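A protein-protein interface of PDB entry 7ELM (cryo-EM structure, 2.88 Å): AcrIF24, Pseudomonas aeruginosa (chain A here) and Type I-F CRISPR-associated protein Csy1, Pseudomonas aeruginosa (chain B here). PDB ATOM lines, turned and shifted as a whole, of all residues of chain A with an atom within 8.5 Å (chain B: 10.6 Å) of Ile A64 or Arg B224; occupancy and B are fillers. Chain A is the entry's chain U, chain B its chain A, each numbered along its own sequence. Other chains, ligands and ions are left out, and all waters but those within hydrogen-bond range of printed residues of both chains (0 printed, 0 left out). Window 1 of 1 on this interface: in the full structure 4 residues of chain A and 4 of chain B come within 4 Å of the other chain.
The side-chain carboxylate of Glu B226 lies within salt-bridge range of the guanidinium group of Arg A67 (3.8 Å).
Ala A60 touches Ser B223. Ala A60 touches Arg B224 (CB to NE, 3.4 Å). Arg B224 touches Val A63. Arg B224 touches Ile A64 (CG to CD1, 3.8 Å). Ile A64 touches Gln B225 (CD1 to OE1, 3.3 Å). Arg B224 touches Arg A67 (CG to NH2, 3.4 Å).
Of chain B, only Ser B223 (3.4 Å) and Arg B224 (3.4 Å) come within 4 Å of Ala A60. Val A63 touches one residue of chain B. Ile A64 touches two residues of chain B. No residue of chain B comes within 4 Å of Asp A65. No residue of chain B comes within 4 Å of Ala A66. Ser B223 touches just one residue of chain A: Ala A60. Of the printed residues of chain A, Gln B225 touches Ile A64. Of the printed residues of chain A, Glu B226 touches Arg A67 (3.8 Å). The nearest residue of chain B that does not touch Ile A64 is Ser B223 (4.5 Å). The nearest residue of chain A that does not touch Arg B224 is Ile A59 (4.5 Å). The nearest printed residue of chain A that does not touch Glu B226 is Ile A64 (6.2 Å).
Of the 23 printed residues of chain A, 4 touch a printed residue of chain B. Of the 14 printed residues of chain B, 4 touch a printed residue of chain A. Among the printed residues, 7 pairs touch across the chains.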
ATOM      1  N   ILE A   6     -26.717 -39.434 -24.380  1.00  0.00           N
ATOM      2  CA  ILE A   6     -27.104 -38.740 -23.160  1.00  0.00           C
ATOM      3  C   ILE A   6     -27.969 -37.569 -23.606  1.00  0.00           C
ATOM      4  O   ILE A   6     -27.465 -36.481 -23.898  1.00  0.00           O
ATOM      5  CB  ILE A   6     -25.901 -38.268 -22.345  1.00  0.00           C
ATOM      6  CG1 ILE A   6     -24.929 -39.418 -22.116  1.00  0.00           C
ATOM      7  CG2 ILE A   6     -26.352 -37.708 -21.013  1.00  0.00           C
ATOM      8  CD1 ILE A   6     -23.500 -38.984 -22.086  1.00  0.00           C
ATOM      9  N   PHE A   9     -27.058 -35.410 -26.594  1.00  0.00           N
ATOM     10  CA  PHE A   9     -25.636 -35.601 -26.830  1.00  0.00           C
ATOM     11  C   PHE A   9     -25.347 -37.033 -27.246  1.00  0.00           C
ATOM     12  O   PHE A   9     -25.996 -37.969 -26.778  1.00  0.00           O
ATOM     13  CB  PHE A   9     -24.829 -35.273 -25.578  1.00  0.00           C
ATOM     14  CG  PHE A   9     -25.032 -33.887 -25.085  1.00  0.00           C
ATOM     15  CD1 PHE A   9     -24.389 -32.827 -25.688  1.00  0.00           C
ATOM     16  CD2 PHE A   9     -25.863 -33.641 -24.012  1.00  0.00           C
ATOM     17  CE1 PHE A   9     -24.573 -31.551 -25.232  1.00  0.00           C
ATOM     18  CE2 PHE A   9     -26.052 -32.365 -23.555  1.00  0.00           C
ATOM     19  CZ  PHE A   9     -25.405 -31.321 -24.165  1.00  0.00           C
ATOM     20  N   PHE A  55     -17.145 -37.135 -20.034  1.00  0.00           N
ATOM     21  CA  PHE A  55     -17.694 -35.993 -20.758  1.00  0.00           C
ATOM     22  C   PHE A  55     -18.785 -35.265 -19.986  1.00  0.00           C
ATOM     23  O   PHE A  55     -19.331 -34.267 -20.492  1.00  0.00           O
ATOM     24  CB  PHE A  55     -18.254 -36.442 -22.107  1.00  0.00           C
ATOM     25  CG  PHE A  55     -17.214 -36.915 -23.072  1.00  0.00           C
ATOM     26  CD1 PHE A  55     -16.584 -36.027 -23.922  1.00  0.00           C
ATOM     27  CD2 PHE A  55     -16.882 -38.251 -23.147  1.00  0.00           C
ATOM     28  CE1 PHE A  55     -15.636 -36.464 -24.820  1.00  0.00           C
ATOM     29  CE2 PHE A  55     -15.936 -38.693 -24.041  1.00  0.00           C
ATOM     30  CZ  PHE A  55     -15.311 -37.797 -24.877  1.00  0.00           C
ATOM     31  N   SER A  56     -19.134 -35.768 -18.795  1.00  0.00           N
ATOM     32  CA  SER A  56     -20.157 -35.130 -17.968  1.00  0.00           C
ATOM     33  C   SER A  56     -19.827 -33.684 -17.609  1.00  0.00           C
ATOM     34  O   SER A  56     -20.740 -32.866 -17.479  1.00  0.00           O
ATOM     35  CB  SER A  56     -20.366 -35.934 -16.691  1.00  0.00           C
ATOM     36  OG  SER A  56     -19.467 -35.508 -15.688  1.00  0.00           O
ATOM     37  N   ASP A  57     -18.543 -33.340 -17.471  1.00  0.00           N
ATOM     38  CA  ASP A  57     -18.182 -31.967 -17.121  1.00  0.00           C
ATOM     39  C   ASP A  57     -18.444 -31.004 -18.275  1.00  0.00           C
ATOM     40  O   ASP A  57     -18.917 -29.882 -18.060  1.00  0.00           O
ATOM     41  CB  ASP A  57     -16.722 -31.893 -16.699  1.00  0.00           C
ATOM     42  CG  ASP A  57     -16.542 -32.107 -15.218  1.00  0.00           C
ATOM     43  OD1 ASP A  57     -17.539 -31.973 -14.481  1.00  0.00           O
ATOM     44  OD2 ASP A  57     -15.412 -32.410 -14.791  1.00  0.00           O
ATOM     45  N   ILE A  58     -18.153 -31.426 -19.504  1.00  0.00           N
ATOM     46  CA  ILE A  58     -18.429 -30.590 -20.667  1.00  0.00           C
ATOM     47  C   ILE A  58     -19.929 -30.447 -20.867  1.00  0.00           C
ATOM     48  O   ILE A  58     -20.422 -29.370 -21.229  1.00  0.00           O
ATOM     49  CB  ILE A  58     -17.747 -31.176 -21.912  1.00  0.00           C
ATOM     50  CG1 ILE A  58     -16.408 -31.794 -21.528  1.00  0.00           C
ATOM     51  CG2 ILE A  58     -17.553 -30.104 -22.953  1.00  0.00           C
ATOM     52  CD1 ILE A  58     -15.671 -32.416 -22.674  1.00  0.00           C
ATOM     53  N   ILE A  59     -20.676 -31.522 -20.600  1.00  0.00           N
ATOM     54  CA  ILE A  59     -22.133 -31.454 -20.675  1.00  0.00           C
ATOM     55  C   ILE A  59     -22.688 -30.497 -19.620  1.00  0.00           C
ATOM     56  O   ILE A  59     -23.593 -29.699 -19.899  1.00  0.00           O
ATOM     57  CB  ILE A  59     -22.722 -32.870 -20.550  1.00  0.00           C
ATOM     58  CG1 ILE A  59     -22.328 -33.697 -21.769  1.00  0.00           C
ATOM     59  CG2 ILE A  59     -24.229 -32.835 -20.426  1.00  0.00           C
ATOM     60  CD1 ILE A  59     -22.726 -35.137 -21.678  1.00  0.00           C
ATOM     61  N   ALA A  60     -22.112 -30.515 -18.416  1.00  0.00           N
ATOM     62  CA  ALA A  60     -22.572 -29.630 -17.352  1.00  0.00           C
ATOM     63  C   ALA A  60     -22.252 -28.172 -17.654  1.00  0.00           C
ATOM     64  O   ALA A  60     -23.052 -27.283 -17.346  1.00  0.00           O
ATOM     65  CB  ALA A  60     -21.947 -30.048 -16.027  1.00  0.00           C
ATOM     66  N   GLU A  61     -21.093 -27.909 -18.262  1.00  0.00           N
ATOM     67  CA  GLU A  61     -20.773 -26.545 -18.674  1.00  0.00           C
ATOM     68  C   GLU A  61     -21.708 -26.061 -19.774  1.00  0.00           C
ATOM     69  O   GLU A  61     -22.094 -24.885 -19.790  1.00  0.00           O
ATOM     70  CB  GLU A  61     -19.324 -26.451 -19.135  1.00  0.00           C
ATOM     71  CG  GLU A  61     -18.310 -26.571 -18.029  1.00  0.00           C
ATOM     72  CD  GLU A  61     -16.896 -26.448 -18.547  1.00  0.00           C
ATOM     73  OE1 GLU A  61     -16.676 -25.636 -19.468  1.00  0.00           O
ATOM     74  OE2 GLU A  61     -16.000 -27.145 -18.025  1.00  0.00           O
ATOM     75  N   PHE A  62     -22.082 -26.952 -20.699  1.00  0.00           N
ATOM     76  CA  PHE A  62     -23.079 -26.603 -21.709  1.00  0.00           C
ATOM     77  C   PHE A  62     -24.417 -26.262 -21.068  1.00  0.00           C
ATOM     78  O   PHE A  62     -25.095 -25.324 -21.500  1.00  0.00           O
ATOM     79  CB  PHE A  62     -23.248 -27.751 -22.703  1.00  0.00           C
ATOM     80  CG  PHE A  62     -24.215 -27.460 -23.819  1.00  0.00           C
ATOM     81  CD1 PHE A  62     -23.796 -26.785 -24.945  1.00  0.00           C
ATOM     82  CD2 PHE A  62     -25.536 -27.872 -23.749  1.00  0.00           C
ATOM     83  CE1 PHE A  62     -24.672 -26.515 -25.971  1.00  0.00           C
ATOM     84  CE2 PHE A  62     -26.413 -27.603 -24.768  1.00  0.00           C
ATOM     85  CZ  PHE A  62     -25.981 -26.925 -25.882  1.00  0.00           C
ATOM     86  N   VAL A  63     -24.803 -27.012 -20.036  1.00  0.00           N
ATOM     87  CA  VAL A  63     -26.080 -26.775 -19.366  1.00  0.00           C
ATOM     88  C   VAL A  63     -26.063 -25.442 -18.628  1.00  0.00           C
ATOM     89  O   VAL A  63     -27.034 -24.680 -18.689  1.00  0.00           O
ATOM     90  CB  VAL A  63     -26.405 -27.957 -18.434  1.00  0.00           C
ATOM     91  CG1 VAL A  63     -27.507 -27.612 -17.451  1.00  0.00           C
ATOM     92  CG2 VAL A  63     -26.820 -29.152 -19.256  1.00  0.00           C
ATOM     93  N   ILE A  64     -24.947 -25.122 -17.967  1.00  0.00           N
ATOM     94  CA  ILE A  64     -24.801 -23.838 -17.277  1.00  0.00           C
ATOM     95  C   ILE A  64     -24.859 -22.678 -18.264  1.00  0.00           C
ATOM     96  O   ILE A  64     -25.549 -21.676 -18.029  1.00  0.00           O
ATOM     97  CB  ILE A  64     -23.494 -23.818 -16.462  1.00  0.00           C
ATOM     98  CG1 ILE A  64     -23.561 -24.814 -15.308  1.00  0.00           C
ATOM     99  CG2 ILE A  64     -23.203 -22.438 -15.919  1.00  0.00           C
ATOM    100  CD1 ILE A  64     -24.753 -24.638 -14.431  1.00  0.00           C
ATOM    101  N   ASP A  65     -24.173 -22.812 -19.402  1.00  0.00           N
ATOM    102  CA  ASP A  65     -24.160 -21.738 -20.388  1.00  0.00           C
ATOM    103  C   ASP A  65     -25.524 -21.554 -21.040  1.00  0.00           C
ATOM    104  O   ASP A  65     -25.950 -20.420 -21.283  1.00  0.00           O
ATOM    105  CB  ASP A  65     -23.094 -22.012 -21.443  1.00  0.00           C
ATOM    106  CG  ASP A  65     -22.958 -20.884 -22.443  1.00  0.00           C
ATOM    107  OD1 ASP A  65     -23.703 -20.871 -23.446  1.00  0.00           O
ATOM    108  OD2 ASP A  65     -22.106 -20.000 -22.220  1.00  0.00           O
ATOM    109  N   ALA A  66     -26.232 -22.650 -21.318  1.00  0.00           N
ATOM    110  CA  ALA A  66     -27.553 -22.529 -21.922  1.00  0.00           C
ATOM    111  C   ALA A  66     -28.574 -22.009 -20.926  1.00  0.00           C
ATOM    112  O   ALA A  66     -29.515 -21.310 -21.314  1.00  0.00           O
ATOM    113  CB  ALA A  66     -28.000 -23.875 -22.481  1.00  0.00           C
ATOM    114  N   ARG A  67     -28.403 -22.328 -19.645  1.00  0.00           N
ATOM    115  CA  ARG A  67     -29.318 -21.832 -18.632  1.00  0.00           C
ATOM    116  C   ARG A  67     -29.102 -20.353 -18.366  1.00  0.00           C
ATOM    117  O   ARG A  67     -30.063 -19.628 -18.089  1.00  0.00           O
ATOM    118  CB  ARG A  67     -29.142 -22.640 -17.354  1.00  0.00           C
ATOM    119  CG  ARG A  67     -30.175 -22.381 -16.306  1.00  0.00           C
ATOM    120  CD  ARG A  67     -30.422 -23.630 -15.513  1.00  0.00           C
ATOM    121  NE  ARG A  67     -29.198 -24.128 -14.907  1.00  0.00           N
ATOM    122  CZ  ARG A  67     -29.075 -25.337 -14.380  1.00  0.00           C
ATOM    123  NH1 ARG A  67     -30.102 -26.173 -14.388  1.00  0.00           N
ATOM    124  NH2 ARG A  67     -27.926 -25.714 -13.845  1.00  0.00           N
ATOM    125  N   HIS A  68     -27.862 -19.882 -18.455  1.00  0.00           N
ATOM    126  CA  HIS A  68     -27.623 -18.462 -18.244  1.00  0.00           C
ATOM    127  C   HIS A  68     -27.959 -17.646 -19.485  1.00  0.00           C
ATOM    128  O   HIS A  68     -28.433 -16.511 -19.372  1.00  0.00           O
ATOM    129  CB  HIS A  68     -26.172 -18.230 -17.828  1.00  0.00           C
ATOM    130  CG  HIS A  68     -25.769 -16.791 -17.831  1.00  0.00           C
ATOM    131  ND1 HIS A  68     -25.100 -16.209 -18.885  1.00  0.00           N
ATOM    132  CD2 HIS A  68     -25.954 -15.812 -16.915  1.00  0.00           C
ATOM    133  CE1 HIS A  68     -24.883 -14.934 -18.615  1.00  0.00           C
ATOM    134  NE2 HIS A  68     -25.391 -14.668 -17.426  1.00  0.00           N
ATOM    135  N   ARG A  69     -27.731 -18.202 -20.675  1.00  0.00           N
ATOM    136  CA  ARG A  69     -27.920 -17.432 -21.897  1.00  0.00           C
ATOM    137  C   ARG A  69     -29.393 -17.233 -22.214  1.00  0.00           C
ATOM    138  O   ARG A  69     -29.815 -16.130 -22.575  1.00  0.00           O
ATOM    139  CB  ARG A  69     -27.217 -18.123 -23.061  1.00  0.00           C
ATOM    140  CG  ARG A  69     -27.440 -17.458 -24.401  1.00  0.00           C
ATOM    141  CD  ARG A  69     -26.920 -18.318 -25.526  1.00  0.00           C
ATOM    142  NE  ARG A  69     -25.635 -18.911 -25.184  1.00  0.00           N
ATOM    143  CZ  ARG A  69     -24.464 -18.325 -25.402  1.00  0.00           C
ATOM    144  NH1 ARG A  69     -24.413 -17.127 -25.968  1.00  0.00           N
ATOM    145  NH2 ARG A  69     -23.342 -18.937 -25.054  1.00  0.00           N
ATOM    146  N   TYR A  70     -30.195 -18.287 -22.082  1.00  0.00           N
ATOM    147  CA  TYR A  70     -31.613 -18.237 -22.404  1.00  0.00           C
ATOM    148  C   TYR A  70     -32.481 -18.053 -21.169  1.00  0.00           C
ATOM    149  O   TYR A  70     -33.604 -18.561 -21.123  1.00  0.00           O
ATOM    150  CB  TYR A  70     -32.022 -19.499 -23.154  1.00  0.00           C
ATOM    151  CG  TYR A  70     -31.199 -19.753 -24.381  1.00  0.00           C
ATOM    152  CD1 TYR A  70     -31.281 -18.908 -25.474  1.00  0.00           C
ATOM    153  CD2 TYR A  70     -30.341 -20.838 -24.453  1.00  0.00           C
ATOM    154  CE1 TYR A  70     -30.536 -19.134 -26.602  1.00  0.00           C
ATOM    155  CE2 TYR A  70     -29.590 -21.073 -25.579  1.00  0.00           C
ATOM    156  CZ  TYR A  70     -29.693 -20.216 -26.650  1.00  0.00           C
ATOM    157  OH  TYR A  70     -28.945 -20.441 -27.780  1.00  0.00           O
ATOM    158  N   ALA A  71     -31.976 -17.349 -20.165  1.00  0.00           N
ATOM    159  CA  ALA A  71     -32.777 -17.047 -18.995  1.00  0.00           C
ATOM    160  C   ALA A  71     -33.879 -16.060 -19.366  1.00  0.00           C
ATOM    161  O   ALA A  71     -33.662 -15.172 -20.195  1.00  0.00           O
ATOM    162  CB  ALA A  71     -31.904 -16.466 -17.889  1.00  0.00           C
ATOM    163  N   TRP A 142     -35.741 -21.973 -20.169  1.00  0.00           N
ATOM    164  CA  TRP A 142     -34.516 -21.795 -20.938  1.00  0.00           C
ATOM    165  C   TRP A 142     -34.317 -22.871 -21.994  1.00  0.00           C
ATOM    166  O   TRP A 142     -33.592 -22.635 -22.966  1.00  0.00           O
ATOM    167  CB  TRP A 142     -33.314 -21.761 -20.002  1.00  0.00           C
ATOM    168  CG  TRP A 142     -33.156 -22.982 -19.171  1.00  0.00           C
ATOM    169  CD1 TRP A 142     -33.677 -23.199 -17.938  1.00  0.00           C
ATOM    170  CD2 TRP A 142     -32.409 -24.153 -19.503  1.00  0.00           C
ATOM    171  NE1 TRP A 142     -33.311 -24.435 -17.480  1.00  0.00           N
ATOM    172  CE2 TRP A 142     -32.530 -25.042 -18.425  1.00  0.00           C
ATOM    173  CE3 TRP A 142     -31.653 -24.540 -20.611  1.00  0.00           C
ATOM    174  CZ2 TRP A 142     -31.925 -26.289 -18.419  1.00  0.00           C
ATOM    175  CZ3 TRP A 142     -31.054 -25.778 -20.602  1.00  0.00           C
ATOM    176  CH2 TRP A 142     -31.191 -26.638 -19.515  1.00  0.00           C
ATOM    177  N   GLY A 174     -31.436 -38.503 -20.031  1.00  0.00           N
ATOM    178  CA  GLY A 174     -30.368 -37.559 -20.245  1.00  0.00           C
ATOM    179  C   GLY A 174     -30.823 -36.195 -20.687  1.00  0.00           C
ATOM    180  O   GLY A 174     -29.987 -35.335 -20.976  1.00  0.00           O
ATOM    181  N   SER A 175     -32.130 -35.970 -20.755  1.00  0.00           N
ATOM    182  CA  SER A 175     -32.665 -34.709 -21.232  1.00  0.00           C
ATOM    183  C   SER A 175     -32.487 -33.615 -20.184  1.00  0.00           C
ATOM    184  O   SER A 175     -32.094 -33.860 -19.042  1.00  0.00           O
ATOM    185  CB  SER A 175     -34.138 -34.861 -21.586  1.00  0.00           C
ATOM    186  OG  SER A 175     -34.840 -35.468 -20.520  1.00  0.00           O
ATOM    187  N   PHE A 176     -32.797 -32.387 -20.588  1.00  0.00           N
ATOM    188  CA  PHE A 176     -32.620 -31.248 -19.703  1.00  0.00           C
ATOM    189  C   PHE A 176     -33.728 -31.134 -18.670  1.00  0.00           C
ATOM    190  O   PHE A 176     -33.545 -30.446 -17.664  1.00  0.00           O
ATOM    191  CB  PHE A 176     -32.532 -29.967 -20.525  1.00  0.00           C
ATOM    192  CG  PHE A 176     -31.428 -29.980 -21.534  1.00  0.00           C
ATOM    193  CD1 PHE A 176     -30.150 -30.353 -21.169  1.00  0.00           C
ATOM    194  CD2 PHE A 176     -31.672 -29.638 -22.848  1.00  0.00           C
ATOM    195  CE1 PHE A 176     -29.135 -30.372 -22.095  1.00  0.00           C
ATOM    196  CE2 PHE A 176     -30.659 -29.659 -23.779  1.00  0.00           C
ATOM    197  CZ  PHE A 176     -29.392 -30.023 -23.400  1.00  0.00           C
ATOM    198  N   LYS B 216     -21.661 -38.624  -4.620  1.00  0.00           N
ATOM    199  CA  LYS B 216     -21.903 -38.435  -6.049  1.00  0.00           C
ATOM    200  C   LYS B 216     -23.091 -37.514  -6.288  1.00  0.00           C
ATOM    201  O   LYS B 216     -23.068 -36.684  -7.204  1.00  0.00           O
ATOM    202  CB  LYS B 216     -22.135 -39.780  -6.741  1.00  0.00           C
ATOM    203  CG  LYS B 216     -21.152 -40.876  -6.368  1.00  0.00           C
ATOM    204  CD  LYS B 216     -20.056 -41.053  -7.399  1.00  0.00           C
ATOM    205  CE  LYS B 216     -19.447 -42.442  -7.278  1.00  0.00           C
ATOM    206  NZ  LYS B 216     -17.998 -42.472  -7.610  1.00  0.00           N
ATOM    207  N   ALA B 217     -24.130 -37.630  -5.456  1.00  0.00           N
ATOM    208  CA  ALA B 217     -25.297 -36.765  -5.592  1.00  0.00           C
ATOM    209  C   ALA B 217     -24.966 -35.324  -5.226  1.00  0.00           C
ATOM    210  O   ALA B 217     -25.420 -34.389  -5.898  1.00  0.00           O
ATOM    211  CB  ALA B 217     -26.437 -37.295  -4.724  1.00  0.00           C
ATOM    212  N   ALA B 218     -24.154 -35.122  -4.186  1.00  0.00           N
ATOM    213  CA  ALA B 218     -23.752 -33.765  -3.824  1.00  0.00           C
ATOM    214  C   ALA B 218     -22.794 -33.175  -4.852  1.00  0.00           C
ATOM    215  O   ALA B 218     -22.855 -31.974  -5.145  1.00  0.00           O
ATOM    216  CB  ALA B 218     -23.125 -33.756  -2.433  1.00  0.00           C
ATOM    217  N   ARG B 219     -21.925 -34.004  -5.437  1.00  0.00           N
ATOM    218  CA  ARG B 219     -21.036 -33.528  -6.491  1.00  0.00           C
ATOM    219  C   ARG B 219     -21.802 -33.189  -7.763  1.00  0.00           C
ATOM    220  O   ARG B 219     -21.424 -32.256  -8.477  1.00  0.00           O
ATOM    221  CB  ARG B 219     -19.961 -34.574  -6.782  1.00  0.00           C
ATOM    222  N   GLU B 220     -22.878 -33.921  -8.056  1.00  0.00           N
ATOM    223  CA  GLU B 220     -23.714 -33.570  -9.198  1.00  0.00           C
ATOM    224  C   GLU B 220     -24.518 -32.305  -8.924  1.00  0.00           C
ATOM    225  O   GLU B 220     -24.679 -31.461  -9.811  1.00  0.00           O
ATOM    226  CB  GLU B 220     -24.641 -34.733  -9.546  1.00  0.00           C
ATOM    227  N   ALA B 221     -25.021 -32.149  -7.698  1.00  0.00           N
ATOM    228  CA  ALA B 221     -25.788 -30.965  -7.335  1.00  0.00           C
ATOM    229  C   ALA B 221     -24.921 -29.732  -7.129  1.00  0.00           C
ATOM    230  O   ALA B 221     -25.466 -28.630  -7.010  1.00  0.00           O
ATOM    231  CB  ALA B 221     -26.601 -31.230  -6.067  1.00  0.00           C
ATOM    232  N   ARG B 222     -23.601 -29.890  -7.038  1.00  0.00           N
ATOM    233  CA  ARG B 222     -22.693 -28.753  -7.041  1.00  0.00           C
ATOM    234  C   ARG B 222     -21.964 -28.565  -8.361  1.00  0.00           C
ATOM    235  O   ARG B 222     -21.332 -27.521  -8.551  1.00  0.00           O
ATOM    236  CB  ARG B 222     -21.663 -28.883  -5.915  1.00  0.00           C
ATOM    237  N   SER B 223     -22.014 -29.546  -9.266  1.00  0.00           N
ATOM    238  CA  SER B 223     -21.494 -29.336 -10.612  1.00  0.00           C
ATOM    239  C   SER B 223     -22.366 -28.358 -11.381  1.00  0.00           C
ATOM    240  O   SER B 223     -21.870 -27.625 -12.245  1.00  0.00           O
ATOM    241  CB  SER B 223     -21.396 -30.666 -11.357  1.00  0.00           C
ATOM    242  OG  SER B 223     -21.287 -30.456 -12.752  1.00  0.00           O
ATOM    243  N   ARG B 224     -23.657 -28.345 -11.090  1.00  0.00           N
ATOM    244  CA  ARG B 224     -24.564 -27.274 -11.460  1.00  0.00           C
ATOM    245  C   ARG B 224     -24.925 -26.522 -10.184  1.00  0.00           C
ATOM    246  O   ARG B 224     -24.523 -26.900  -9.084  1.00  0.00           O
ATOM    247  CB  ARG B 224     -25.805 -27.817 -12.177  1.00  0.00           C
ATOM    248  CG  ARG B 224     -25.626 -28.215 -13.648  1.00  0.00           C
ATOM    249  CD  ARG B 224     -24.966 -29.575 -13.816  1.00  0.00           C
ATOM    250  NE  ARG B 224     -25.186 -30.169 -15.132  1.00  0.00           N
ATOM    251  CZ  ARG B 224     -26.174 -31.008 -15.426  1.00  0.00           C
ATOM    252  NH1 ARG B 224     -27.049 -31.356 -14.496  1.00  0.00           N
ATOM    253  NH2 ARG B 224     -26.280 -31.499 -16.653  1.00  0.00           N
ATOM    254  N   GLN B 225     -25.685 -25.440 -10.319  1.00  0.00           N
ATOM    255  CA  GLN B 225     -25.949 -24.566  -9.183  1.00  0.00           C
ATOM    256  C   GLN B 225     -27.317 -24.799  -8.546  1.00  0.00           C
ATOM    257  O   GLN B 225     -27.964 -23.840  -8.117  1.00  0.00           O
ATOM    258  CB  GLN B 225     -25.797 -23.100  -9.592  1.00  0.00           C
ATOM    259  CG  GLN B 225     -24.381 -22.523  -9.485  1.00  0.00           C
ATOM    260  CD  GLN B 225     -23.435 -22.910 -10.615  1.00  0.00           C
ATOM    261  OE1 GLN B 225     -23.706 -23.805 -11.410  1.00  0.00           O
ATOM    262  NE2 GLN B 225     -22.313 -22.207 -10.693  1.00  0.00           N
ATOM    263  N   GLU B 226     -27.771 -26.047  -8.459  1.00  0.00           N
ATOM    264  CA  GLU B 226     -28.974 -26.332  -7.692  1.00  0.00           C
ATOM    265  C   GLU B 226     -28.632 -26.549  -6.218  1.00  0.00           C
ATOM    266  O   GLU B 226     -27.473 -26.477  -5.798  1.00  0.00           O
ATOM    267  CB  GLU B 226     -29.718 -27.544  -8.251  1.00  0.00           C
ATOM    268  CG  GLU B 226     -28.840 -28.729  -8.596  1.00  0.00           C
ATOM    269  CD  GLU B 226     -28.468 -28.748 -10.061  1.00  0.00           C
ATOM    270  OE1 GLU B 226     -27.968 -29.787 -10.541  1.00  0.00           O
ATOM    271  OE2 GLU B 226     -28.719 -27.731 -10.740  1.00  0.00           O
ATOM    272  N   SER B 227     -29.662 -26.823  -5.424  1.00  0.00           N
ATOM    273  CA  SER B 227     -29.535 -26.998  -3.986  1.00  0.00           C
ATOM    274  C   SER B 227     -29.436 -28.476  -3.620  1.00  0.00           C
ATOM    275  O   SER B 227     -29.832 -29.360  -4.381  1.00  0.00           O
ATOM    276  CB  SER B 227     -30.720 -26.360  -3.257  1.00  0.00           C
ATOM    277  N   TRP B 228     -28.897 -28.724  -2.425  1.00  0.00           N
ATOM    278  CA  TRP B 228     -28.752 -30.055  -1.846  1.00  0.00           C
ATOM    279  C   TRP B 228     -28.572 -29.906  -0.342  1.00  0.00           C
ATOM    280  O   TRP B 228     -27.717 -29.130   0.101  1.00  0.00           O
ATOM    281  CB  TRP B 228     -27.567 -30.798  -2.466  1.00  0.00           C
ATOM    282  CG  TRP B 228     -27.661 -32.291  -2.361  1.00  0.00           C
ATOM    283  CD1 TRP B 228     -26.828 -33.115  -1.662  1.00  0.00           C
ATOM    284  CD2 TRP B 228     -28.641 -33.140  -2.975  1.00  0.00           C
ATOM    285  NE1 TRP B 228     -27.225 -34.421  -1.804  1.00  0.00           N
ATOM    286  CE2 TRP B 228     -28.337 -34.463  -2.604  1.00  0.00           C
ATOM    287  CE3 TRP B 228     -29.743 -32.910  -3.803  1.00  0.00           C
ATOM    288  CZ2 TRP B 228     -29.097 -35.549  -3.029  1.00  0.00           C
ATOM    289  CZ3 TRP B 228     -30.494 -33.989  -4.222  1.00  0.00           C
ATOM    290  CH2 TRP B 228     -30.168 -35.292  -3.837  1.00  0.00           C
ATOM    291  N   PHE B 232     -20.412 -31.767   0.503  1.00  0.00           N
ATOM    292  CA  PHE B 232     -19.494 -32.867   0.237  1.00  0.00           C
ATOM    293  C   PHE B 232     -18.065 -32.408   0.488  1.00  0.00           C
ATOM    294  O   PHE B 232     -17.840 -31.269   0.908  1.00  0.00           O
ATOM    295  CB  PHE B 232     -19.663 -33.396  -1.193  1.00  0.00           C
ATOM    296  CG  PHE B 232     -19.183 -32.450  -2.262  1.00  0.00           C
ATOM    297  CD1 PHE B 232     -19.938 -31.346  -2.624  1.00  0.00           C
ATOM    298  CD2 PHE B 232     -17.992 -32.680  -2.926  1.00  0.00           C
ATOM    299  CE1 PHE B 232     -19.501 -30.481  -3.595  1.00  0.00           C
ATOM    300  CE2 PHE B 232     -17.558 -31.814  -3.909  1.00  0.00           C
ATOM    301  CZ  PHE B 232     -18.311 -30.717  -4.242  1.00  0.00           C
